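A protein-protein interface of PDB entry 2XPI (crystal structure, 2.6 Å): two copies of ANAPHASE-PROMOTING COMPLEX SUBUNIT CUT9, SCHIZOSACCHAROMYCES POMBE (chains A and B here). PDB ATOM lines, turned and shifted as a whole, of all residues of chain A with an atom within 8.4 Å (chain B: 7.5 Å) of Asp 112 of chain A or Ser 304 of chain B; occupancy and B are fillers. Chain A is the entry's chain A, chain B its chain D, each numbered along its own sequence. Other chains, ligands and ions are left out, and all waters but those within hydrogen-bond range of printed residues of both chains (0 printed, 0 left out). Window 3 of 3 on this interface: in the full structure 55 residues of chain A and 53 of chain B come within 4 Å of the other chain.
The side-chain amino group of Lys 109 of chain A is in hydrogen-bond range of the side-chain hydroxyl of Ser 304 of chain B (3.4 Å). The side-chain amino group (NZ) of Lys 109 of chain A is in salt-bridge range of the side-chain carboxylate (OD2) of Asp 306 of chain B (3.2 Å).
The side-chain carboxylate of Glu 302 of chain B lies within hydrogen-bond range of the backbone NH of Gly 300 of chain B (3.3 Å).
No position is printed for both chains. Of the 6 pairs that touch across the chains among the printed residues, none has its exchanged pair printed and touching as well.
Of the 18 printed residues of chain A, 4 touch a printed residue of chain B. Among the printed residues, 6 pairs touch across the chains. Among the printed residues, Asp or Glu carboxylates within 4 Å of a Lys or Arg side-chain nitrogen of the other chain: Lys 109 of chain A with Asp 306 of chain B.
Among the printed residues, merely in contact across the chains: Phe 105 of chain A with Asp 306 of chain B (3.1 Å), Asp 112 of chain A with Gly 300 of chain B (3.2 Å), Asp 112 of chain A with Ser 304 of chain B (3.3 Å) and Ile 113 of chain A with Asn 299 of chain B (3.9 Å).
Printed residues of chain B within 4 Å of Phe 105 of chain A: Asp 306. Of the printed residues of chain B, Lys 109 of chain A touches Ser 304 (3.4 Å) and Asp 306 (3.1 Å). Printed residues of chain B within 4 Å of Asp 112 of chain A: Gly 300 (3.2 Å) and Ser 304 (3.3 Å). Of the printed residues of chain B, Ile 113 of chain A touches Asn 299. Leu 274 of chain B touches none of the printed residues of chain A. Of the printed residues of chain A, Asn 299 of chain B touches Ile 113. No residue of chain A comes within 4 Å of Lys 303 of chain B. Ser 304 of chain B touches just these residues of chain A: Lys 109 (3.4 Å) and Asp 112 (3.3 Å). No residue of chain A comes within 4 Å of Ser 305 of chain B. Of the printed residues of chain A, Asp 306 of chain B touches Phe 105 (3.1 Å) and Lys 109 (3.1 Å). Leu 309 of chain B touches none of the printed residues of chain A. The nearest residue of chain A that does not touch Ser 304 of chain B is Glu 108 of chain A (6.0 Å).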
ATOM      1  N   LEU A  87       1.704  -6.670   7.669  1.00  0.00           N
ATOM      2  CA  LEU A  87       1.888  -6.641   6.227  1.00  0.00           C
ATOM      3  C   LEU A  87       2.962  -7.638   5.820  1.00  0.00           C
ATOM      4  O   LEU A  87       2.760  -8.462   4.939  1.00  0.00           O
ATOM      5  CB  LEU A  87       2.275  -5.229   5.776  1.00  0.00           C
ATOM      6  CG  LEU A  87       1.112  -4.374   5.249  1.00  0.00           C
ATOM      7  CD1 LEU A  87      -0.155  -4.660   6.011  1.00  0.00           C
ATOM      8  CD2 LEU A  87       1.443  -2.887   5.256  1.00  0.00           C
ATOM      9  N   ALA A 104       3.021  -9.464  -4.225  1.00  0.00           N
ATOM     10  CA  ALA A 104       3.392  -8.218  -4.894  1.00  0.00           C
ATOM     11  C   ALA A 104       2.509  -7.085  -4.400  1.00  0.00           C
ATOM     12  O   ALA A 104       2.988  -5.990  -4.159  1.00  0.00           O
ATOM     13  CB  ALA A 104       3.274  -8.358  -6.408  1.00  0.00           C
ATOM     14  N   PHE A 105       1.219  -7.352  -4.228  1.00  0.00           N
ATOM     15  CA  PHE A 105       0.311  -6.326  -3.743  1.00  0.00           C
ATOM     16  C   PHE A 105       0.674  -5.845  -2.343  1.00  0.00           C
ATOM     17  O   PHE A 105       0.697  -4.643  -2.079  1.00  0.00           O
ATOM     18  CB  PHE A 105      -1.128  -6.835  -3.761  1.00  0.00           C
ATOM     19  CG  PHE A 105      -2.128  -5.839  -3.259  1.00  0.00           C
ATOM     20  CD1 PHE A 105      -2.430  -4.705  -3.999  1.00  0.00           C
ATOM     21  CD2 PHE A 105      -2.782  -6.038  -2.051  1.00  0.00           C
ATOM     22  CE1 PHE A 105      -3.375  -3.773  -3.532  1.00  0.00           C
ATOM     23  CE2 PHE A 105      -3.727  -5.126  -1.586  1.00  0.00           C
ATOM     24  CZ  PHE A 105      -4.022  -3.990  -2.322  1.00  0.00           C
ATOM     25  N   VAL A 106       0.951  -6.780  -1.442  1.00  0.00           N
ATOM     26  CA  VAL A 106       1.232  -6.408  -0.056  1.00  0.00           C
ATOM     27  C   VAL A 106       2.636  -5.860   0.062  1.00  0.00           C
ATOM     28  O   VAL A 106       2.864  -4.883   0.776  1.00  0.00           O
ATOM     29  CB  VAL A 106       1.043  -7.590   0.912  1.00  0.00           C
ATOM     30  CG1 VAL A 106       1.348  -7.173   2.322  1.00  0.00           C
ATOM     31  CG2 VAL A 106      -0.371  -8.124   0.809  1.00  0.00           C
ATOM     32  N   GLY A 107       3.569  -6.493  -0.658  1.00  0.00           N
ATOM     33  CA  GLY A 107       4.968  -6.102  -0.657  1.00  0.00           C
ATOM     34  C   GLY A 107       5.183  -4.697  -1.185  1.00  0.00           C
ATOM     35  O   GLY A 107       6.036  -3.970  -0.698  1.00  0.00           O
ATOM     36  N   GLU A 108       4.410  -4.319  -2.193  1.00  0.00           N
ATOM     37  CA  GLU A 108       4.462  -2.966  -2.714  1.00  0.00           C
ATOM     38  C   GLU A 108       3.960  -1.934  -1.677  1.00  0.00           C
ATOM     39  O   GLU A 108       4.517  -0.839  -1.570  1.00  0.00           O
ATOM     40  CB  GLU A 108       3.708  -2.872  -4.054  1.00  0.00           C
ATOM     41  CG  GLU A 108       4.389  -3.639  -5.213  1.00  0.00           C
ATOM     42  CD  GLU A 108       3.425  -4.055  -6.348  1.00  0.00           C
ATOM     43  OE1 GLU A 108       2.217  -3.684  -6.280  1.00  0.00           O
ATOM     44  OE2 GLU A 108       3.875  -4.759  -7.298  1.00  0.00           O
ATOM     45  N   LYS A 109       2.942  -2.279  -0.895  1.00  0.00           N
ATOM     46  CA  LYS A 109       2.439  -1.340   0.128  1.00  0.00           C
ATOM     47  C   LYS A 109       3.374  -1.113   1.324  1.00  0.00           C
ATOM     48  O   LYS A 109       3.474   0.012   1.814  1.00  0.00           O
ATOM     49  CB  LYS A 109       1.043  -1.723   0.616  1.00  0.00           C
ATOM     50  CG  LYS A 109      -0.061  -1.063  -0.180  1.00  0.00           C
ATOM     51  CD  LYS A 109      -0.740  -2.035  -1.118  1.00  0.00           C
ATOM     52  CE  LYS A 109      -1.033  -1.379  -2.461  1.00  0.00           C
ATOM     53  NZ  LYS A 109       0.230  -0.994  -3.196  1.00  0.00           N
ATOM     54  N   VAL A 110       4.056  -2.164   1.787  1.00  0.00           N
ATOM     55  CA  VAL A 110       5.015  -2.044   2.892  1.00  0.00           C
ATOM     56  C   VAL A 110       6.268  -1.278   2.496  1.00  0.00           C
ATOM     57  O   VAL A 110       6.884  -0.583   3.324  1.00  0.00           O
ATOM     58  CB  VAL A 110       5.527  -3.401   3.364  1.00  0.00           C
ATOM     59  CG1 VAL A 110       6.044  -3.270   4.766  1.00  0.00           C
ATOM     60  CG2 VAL A 110       4.441  -4.455   3.284  1.00  0.00           C
ATOM     61  N   LEU A 111       6.679  -1.446   1.242  1.00  0.00           N
ATOM     62  CA  LEU A 111       7.867  -0.760   0.748  1.00  0.00           C
ATOM     63  C   LEU A 111       7.534   0.720   0.584  1.00  0.00           C
ATOM     64  O   LEU A 111       8.329   1.585   0.960  1.00  0.00           O
ATOM     65  CB  LEU A 111       8.391  -1.380  -0.560  1.00  0.00           C
ATOM     66  CG  LEU A 111       9.655  -0.723  -1.131  1.00  0.00           C
ATOM     67  CD1 LEU A 111      10.794  -0.717  -0.108  1.00  0.00           C
ATOM     68  CD2 LEU A 111      10.113  -1.367  -2.431  1.00  0.00           C
ATOM     69  N   ASP A 112       6.343   1.008   0.051  1.00  0.00           N
ATOM     70  CA  ASP A 112       5.872   2.396  -0.049  1.00  0.00           C
ATOM     71  C   ASP A 112       5.887   3.081   1.317  1.00  0.00           C
ATOM     72  O   ASP A 112       6.342   4.213   1.437  1.00  0.00           O
ATOM     73  CB  ASP A 112       4.480   2.483  -0.695  1.00  0.00           C
ATOM     74  CG  ASP A 112       4.505   2.168  -2.200  1.00  0.00           C
ATOM     75  OD1 ASP A 112       5.571   2.338  -2.844  1.00  0.00           O
ATOM     76  OD2 ASP A 112       3.453   1.751  -2.745  1.00  0.00           O
ATOM     77  N   ILE A 113       5.417   2.386   2.348  1.00  0.00           N
ATOM     78  CA  ILE A 113       5.402   2.943   3.697  1.00  0.00           C
ATOM     79  C   ILE A 113       6.796   3.145   4.310  1.00  0.00           C
ATOM     80  O   ILE A 113       7.123   4.223   4.788  1.00  0.00           O
ATOM     81  CB  ILE A 113       4.579   2.053   4.640  1.00  0.00           C
ATOM     82  CG1 ILE A 113       3.084   2.187   4.342  1.00  0.00           C
ATOM     83  CG2 ILE A 113       4.856   2.404   6.092  1.00  0.00           C
ATOM     84  CD1 ILE A 113       2.247   1.152   5.056  1.00  0.00           C
ATOM     85  N   THR A 114       7.618   2.103   4.265  1.00  0.00           N
ATOM     86  CA  THR A 114       8.831   2.005   5.073  1.00  0.00           C
ATOM     87  C   THR A 114      10.129   2.444   4.370  1.00  0.00           C
ATOM     88  O   THR A 114      11.034   3.019   4.994  1.00  0.00           O
ATOM     89  CB  THR A 114       9.006   0.544   5.536  1.00  0.00           C
ATOM     90  OG1 THR A 114       9.208  -0.292   4.390  1.00  0.00           O
ATOM     91  CG2 THR A 114       7.756   0.076   6.246  1.00  0.00           C
ATOM     92  N   GLY A 115      10.234   2.136   3.081  1.00  0.00           N
ATOM     93  CA  GLY A 115      11.443   2.413   2.335  1.00  0.00           C
ATOM     94  C   GLY A 115      12.602   1.551   2.789  1.00  0.00           C
ATOM     95  O   GLY A 115      13.750   1.811   2.411  1.00  0.00           O
ATOM     96  N   ASN A 116      12.312   0.520   3.587  1.00  0.00           N
ATOM     97  CA  ASN A 116      13.345  -0.391   4.095  1.00  0.00           C
ATOM     98  C   ASN A 116      13.941  -1.314   3.029  1.00  0.00           C
ATOM     99  O   ASN A 116      13.219  -1.988   2.299  1.00  0.00           O
ATOM    100  CB  ASN A 116      12.768  -1.244   5.224  1.00  0.00           C
ATOM    101  CG  ASN A 116      13.839  -1.873   6.106  1.00  0.00           C
ATOM    102  OD1 ASN A 116      13.844  -1.661   7.317  1.00  0.00           O
ATOM    103  ND2 ASN A 116      14.737  -2.652   5.512  1.00  0.00           N
ATOM    104  N   ASP A 119      12.553  -4.683   2.808  1.00  0.00           N
ATOM    105  CA  ASP A 119      11.268  -4.771   2.135  1.00  0.00           C
ATOM    106  C   ASP A 119      11.413  -4.742   0.622  1.00  0.00           C
ATOM    107  O   ASP A 119      10.696  -5.447  -0.081  1.00  0.00           O
ATOM    108  CB  ASP A 119      10.311  -3.702   2.666  1.00  0.00           C
ATOM    109  CG  ASP A 119       9.942  -3.958   4.105  1.00  0.00           C
ATOM    110  OD1 ASP A 119       9.912  -5.154   4.482  1.00  0.00           O
ATOM    111  OD2 ASP A 119       9.719  -2.990   4.866  1.00  0.00           O
ATOM    112  N   ALA A 120      12.357  -3.944   0.133  1.00  0.00           N
ATOM    113  CA  ALA A 120      12.722  -3.954  -1.279  1.00  0.00           C
ATOM    114  C   ALA A 120      13.216  -5.337  -1.684  1.00  0.00           C
ATOM    115  O   ALA A 120      12.881  -5.838  -2.758  1.00  0.00           O
ATOM    116  CB  ALA A 120      13.798  -2.930  -1.547  1.00  0.00           C
ATOM    117  N   LEU A 123      10.229  -7.797  -1.847  1.00  0.00           N
ATOM    118  CA  LEU A 123       9.377  -7.446  -2.980  1.00  0.00           C
ATOM    119  C   LEU A 123      10.052  -7.933  -4.256  1.00  0.00           C
ATOM    120  O   LEU A 123       9.421  -8.548  -5.122  1.00  0.00           O
ATOM    121  CB  LEU A 123       9.176  -5.940  -3.051  1.00  0.00           C
ATOM    122  CG  LEU A 123       7.889  -5.413  -3.690  1.00  0.00           C
ATOM    123  CD1 LEU A 123       8.135  -4.135  -4.492  1.00  0.00           C
ATOM    124  CD2 LEU A 123       7.169  -6.452  -4.533  1.00  0.00           C
ATOM    125  N   LEU A 139      14.072  -2.493  -9.548  1.00  0.00           N
ATOM    126  CA  LEU A 139      13.658  -2.075  -8.223  1.00  0.00           C
ATOM    127  C   LEU A 139      14.865  -1.977  -7.268  1.00  0.00           C
ATOM    128  O   LEU A 139      14.985  -1.026  -6.493  1.00  0.00           O
ATOM    129  CB  LEU A 139      12.607  -3.041  -7.705  1.00  0.00           C
ATOM    130  CG  LEU A 139      12.149  -2.825  -6.271  1.00  0.00           C
ATOM    131  CD1 LEU A 139      11.171  -1.664  -6.223  1.00  0.00           C
ATOM    132  CD2 LEU A 139      11.517  -4.091  -5.729  1.00  0.00           C
ATOM    133  N   LEU B 274      -7.949  -0.142   0.934  1.00  0.00           N
ATOM    134  CA  LEU B 274      -7.102  -0.655  -0.124  1.00  0.00           C
ATOM    135  C   LEU B 274      -7.917  -1.399  -1.170  1.00  0.00           C
ATOM    136  O   LEU B 274      -7.640  -1.288  -2.370  1.00  0.00           O
ATOM    137  CB  LEU B 274      -6.031  -1.583   0.456  1.00  0.00           C
ATOM    138  CG  LEU B 274      -4.583  -1.093   0.579  1.00  0.00           C
ATOM    139  CD1 LEU B 274      -4.522   0.392   0.796  1.00  0.00           C
ATOM    140  CD2 LEU B 274      -3.855  -1.844   1.706  1.00  0.00           C
ATOM    141  N   LEU B 277     -10.064   0.723  -3.528  1.00  0.00           N
ATOM    142  CA  LEU B 277      -9.284   1.288  -4.636  1.00  0.00           C
ATOM    143  C   LEU B 277      -9.391   0.485  -5.933  1.00  0.00           C
ATOM    144  O   LEU B 277      -9.069   0.991  -7.017  1.00  0.00           O
ATOM    145  CB  LEU B 277      -7.807   1.415  -4.265  1.00  0.00           C
ATOM    146  CG  LEU B 277      -7.407   2.384  -3.150  1.00  0.00           C
ATOM    147  CD1 LEU B 277      -5.889   2.540  -3.167  1.00  0.00           C
ATOM    148  CD2 LEU B 277      -8.135   3.765  -3.225  1.00  0.00           C
ATOM    149  N   ILE B 298      -1.630   8.578   5.069  1.00  0.00           N
ATOM    150  CA  ILE B 298      -0.549   7.652   5.430  1.00  0.00           C
ATOM    151  C   ILE B 298       0.685   7.929   4.580  1.00  0.00           C
ATOM    152  O   ILE B 298       0.637   7.820   3.355  1.00  0.00           O
ATOM    153  CB  ILE B 298      -0.980   6.178   5.261  1.00  0.00           C
ATOM    154  CG1 ILE B 298      -2.212   5.876   6.108  1.00  0.00           C
ATOM    155  CG2 ILE B 298       0.138   5.240   5.663  1.00  0.00           C
ATOM    156  CD1 ILE B 298      -2.823   4.529   5.824  1.00  0.00           C
ATOM    157  N   ASN B 299       1.791   8.300   5.222  1.00  0.00           N
ATOM    158  CA  ASN B 299       2.987   8.697   4.474  1.00  0.00           C
ATOM    159  C   ASN B 299       3.611   7.538   3.733  1.00  0.00           C
ATOM    160  O   ASN B 299       3.885   6.489   4.315  1.00  0.00           O
ATOM    161  CB  ASN B 299       4.036   9.420   5.342  1.00  0.00           C
ATOM    162  CG  ASN B 299       3.962   9.045   6.831  1.00  0.00           C
ATOM    163  OD1 ASN B 299       2.899   8.698   7.358  1.00  0.00           O
ATOM    164  ND2 ASN B 299       5.102   9.147   7.519  1.00  0.00           N
ATOM    165  N   GLY B 300       3.819   7.740   2.438  1.00  0.00           N
ATOM    166  CA  GLY B 300       4.430   6.738   1.588  1.00  0.00           C
ATOM    167  C   GLY B 300       3.504   6.294   0.473  1.00  0.00           C
ATOM    168  O   GLY B 300       3.960   5.909  -0.617  1.00  0.00           O
ATOM    169  N   LEU B 301       2.202   6.367   0.749  1.00  0.00           N
ATOM    170  CA  LEU B 301       1.192   5.839  -0.155  1.00  0.00           C
ATOM    171  C   LEU B 301       0.841   6.745  -1.337  1.00  0.00           C
ATOM    172  O   LEU B 301       0.266   6.278  -2.315  1.00  0.00           O
ATOM    173  CB  LEU B 301      -0.052   5.436   0.621  1.00  0.00           C
ATOM    174  CG  LEU B 301       0.183   4.233   1.533  1.00  0.00           C
ATOM    175  CD1 LEU B 301      -1.115   3.795   2.165  1.00  0.00           C
ATOM    176  CD2 LEU B 301       0.790   3.086   0.749  1.00  0.00           C
ATOM    177  N   GLU B 302       1.200   8.025  -1.262  1.00  0.00           N
ATOM    178  CA  GLU B 302       1.028   8.921  -2.405  1.00  0.00           C
ATOM    179  C   GLU B 302       1.860   8.457  -3.604  1.00  0.00           C
ATOM    180  O   GLU B 302       1.615   8.870  -4.738  1.00  0.00           O
ATOM    181  CB  GLU B 302       1.396  10.360  -2.046  1.00  0.00           C
ATOM    182  CG  GLU B 302       2.858  10.574  -1.681  1.00  0.00           C
ATOM    183  CD  GLU B 302       3.182  10.163  -0.247  1.00  0.00           C
ATOM    184  OE1 GLU B 302       2.241   9.980   0.554  1.00  0.00           O
ATOM    185  OE2 GLU B 302       4.379  10.030   0.089  1.00  0.00           O
ATOM    186  N   LYS B 303       2.850   7.605  -3.348  1.00  0.00           N
ATOM    187  CA  LYS B 303       3.738   7.119  -4.401  1.00  0.00           C
ATOM    188  C   LYS B 303       3.235   5.770  -4.907  1.00  0.00           C
ATOM    189  O   LYS B 303       3.762   5.222  -5.870  1.00  0.00           O
ATOM    190  CB  LYS B 303       5.185   7.010  -3.899  1.00  0.00           C
ATOM    191  N   SER B 304       2.198   5.250  -4.255  1.00  0.00           N
ATOM    192  CA  SER B 304       1.617   3.961  -4.623  1.00  0.00           C
ATOM    193  C   SER B 304       0.868   4.005  -5.964  1.00  0.00           C
ATOM    194  O   SER B 304       0.077   4.912  -6.224  1.00  0.00           O
ATOM    195  CB  SER B 304       0.694   3.462  -3.514  1.00  0.00           C
ATOM    196  OG  SER B 304      -0.020   2.321  -3.940  1.00  0.00           O
ATOM    197  N   SER B 305       1.131   3.021  -6.815  1.00  0.00           N
ATOM    198  CA  SER B 305       0.489   2.942  -8.120  1.00  0.00           C
ATOM    199  C   SER B 305      -1.009   2.692  -8.006  1.00  0.00           C
ATOM    200  O   SER B 305      -1.798   3.319  -8.702  1.00  0.00           O
ATOM    201  CB  SER B 305       1.136   1.852  -8.973  1.00  0.00           C
ATOM    202  OG  SER B 305       2.418   2.264  -9.414  1.00  0.00           O
ATOM    203  N   ASP B 306      -1.392   1.771  -7.128  1.00  0.00           N
ATOM    204  CA  ASP B 306      -2.797   1.436  -6.922  1.00  0.00           C
ATOM    205  C   ASP B 306      -3.600   2.659  -6.496  1.00  0.00           C
ATOM    206  O   ASP B 306      -4.725   2.855  -6.945  1.00  0.00           O
ATOM    207  CB  ASP B 306      -2.945   0.331  -5.869  1.00  0.00           C
ATOM    208  CG  ASP B 306      -2.289  -0.973  -6.292  1.00  0.00           C
ATOM    209  OD1 ASP B 306      -2.133  -1.209  -7.509  1.00  0.00           O
ATOM    210  OD2 ASP B 306      -1.933  -1.769  -5.400  1.00  0.00           O
ATOM    211  N   LEU B 307      -3.034   3.473  -5.619  1.00  0.00           N
ATOM    212  CA  LEU B 307      -3.747   4.645  -5.174  1.00  0.00           C
ATOM    213  C   LEU B 307      -3.843   5.607  -6.349  1.00  0.00           C
ATOM    214  O   LEU B 307      -4.936   6.047  -6.726  1.00  0.00           O
ATOM    215  CB  LEU B 307      -3.035   5.307  -3.993  1.00  0.00           C
ATOM    216  CG  LEU B 307      -3.811   6.471  -3.368  1.00  0.00           C
ATOM    217  CD1 LEU B 307      -5.112   5.957  -2.782  1.00  0.00           C
ATOM    218  CD2 LEU B 307      -3.005   7.196  -2.307  1.00  0.00           C
ATOM    219  N   LEU B 308      -2.685   5.910  -6.928  1.00  0.00           N
ATOM    220  CA  LEU B 308      -2.577   6.835  -8.047  1.00  0.00           C
ATOM    221  C   LEU B 308      -3.428   6.419  -9.242  1.00  0.00           C
ATOM    222  O   LEU B 308      -4.019   7.257  -9.920  1.00  0.00           O
ATOM    223  CB  LEU B 308      -1.122   6.943  -8.484  1.00  0.00           C
ATOM    224  CG  LEU B 308      -0.224   7.704  -7.521  1.00  0.00           C
ATOM    225  CD1 LEU B 308       1.190   7.785  -8.093  1.00  0.00           C
ATOM    226  CD2 LEU B 308      -0.787   9.080  -7.287  1.00  0.00           C
ATOM    227  N   LEU B 309      -3.481   5.117  -9.493  1.00  0.00           N
ATOM    228  CA  LEU B 309      -4.189   4.572 -10.632  1.00  0.00           C
ATOM    229  C   LEU B 309      -5.677   4.735 -10.403  1.00  0.00           C
ATOM    230  O   LEU B 309      -6.463   4.889 -11.336  1.00  0.00           O
ATOM    231  CB  LEU B 309      -3.848   3.092 -10.773  1.00  0.00           C
ATOM    232  CG  LEU B 309      -3.864   2.467 -12.161  1.00  0.00           C
ATOM    233  CD1 LEU B 309      -3.903   3.557 -13.210  1.00  0.00           C
ATOM    234  CD2 LEU B 309      -2.634   1.544 -12.346  1.00  0.00           C
ATOM    235  N   CYS B 310      -6.067   4.689  -9.141  1.00  0.00           N
ATOM    236  CA  CYS B 310      -7.455   4.847  -8.789  1.00  0.00           C
ATOM    237  C   CYS B 310      -7.832   6.300  -9.046  1.00  0.00           C
ATOM    238  O   CYS B 310      -8.877   6.589  -9.643  1.00  0.00           O
ATOM    239  CB  CYS B 310      -7.652   4.487  -7.326  1.00  0.00           C
ATOM    240  SG  CYS B 310      -9.349   4.156  -6.849  1.00  0.00           S
ATOM    241  N   ILE B 327      -0.675  12.227 -13.752  1.00  0.00           N
ATOM    242  CA  ILE B 327      -0.510  11.096 -12.848  1.00  0.00           C
ATOM    243  C   ILE B 327       0.090   9.880 -13.577  1.00  0.00           C
ATOM    244  O   ILE B 327       1.140   9.357 -13.202  1.00  0.00           O
ATOM    245  CB  ILE B 327      -1.867  10.701 -12.210  1.00  0.00           C
ATOM    246  CG1 ILE B 327      -2.421  11.842 -11.362  1.00  0.00           C
ATOM    247  CG2 ILE B 327      -1.720   9.444 -11.351  1.00  0.00           C
ATOM    248  CD1 ILE B 327      -3.692  11.483 -10.632  1.00  0.00           C
ATOM    249  N   ILE B 331       3.572   7.709 -13.036  1.00  0.00           N
ATOM    250  CA  ILE B 331       3.637   6.271 -12.825  1.00  0.00           C
ATOM    251  C   ILE B 331       4.634   5.609 -13.768  1.00  0.00           C
ATOM    252  O   ILE B 331       5.363   4.724 -13.356  1.00  0.00           O
ATOM    253  CB  ILE B 331       2.262   5.591 -12.986  1.00  0.00           C
ATOM    254  CG1 ILE B 331       1.324   5.995 -11.850  1.00  0.00           C
ATOM    255  CG2 ILE B 331       2.422   4.084 -13.013  1.00  0.00           C
ATOM    256  CD1 ILE B 331      -0.055   5.412 -11.986  1.00  0.00           C
ATOM    257  N   ILE B 334       8.312   6.423 -12.503  1.00  0.00           N
ATOM    258  CA  ILE B 334       8.712   5.867 -11.202  1.00  0.00           C
ATOM    259  C   ILE B 334       8.443   4.367 -11.030  1.00  0.00           C
ATOM    260  O   ILE B 334       8.699   3.810  -9.964  1.00  0.00           O
ATOM    261  CB  ILE B 334       8.077   6.633 -10.003  1.00  0.00           C
ATOM    262  CG1 ILE B 334       6.596   6.260  -9.848  1.00  0.00           C
ATOM    263  CG2 ILE B 334       8.293   8.140 -10.146  1.00  0.00           C
ATOM    264  CD1 ILE B 334       5.907   6.872  -8.627  1.00  0.00           C
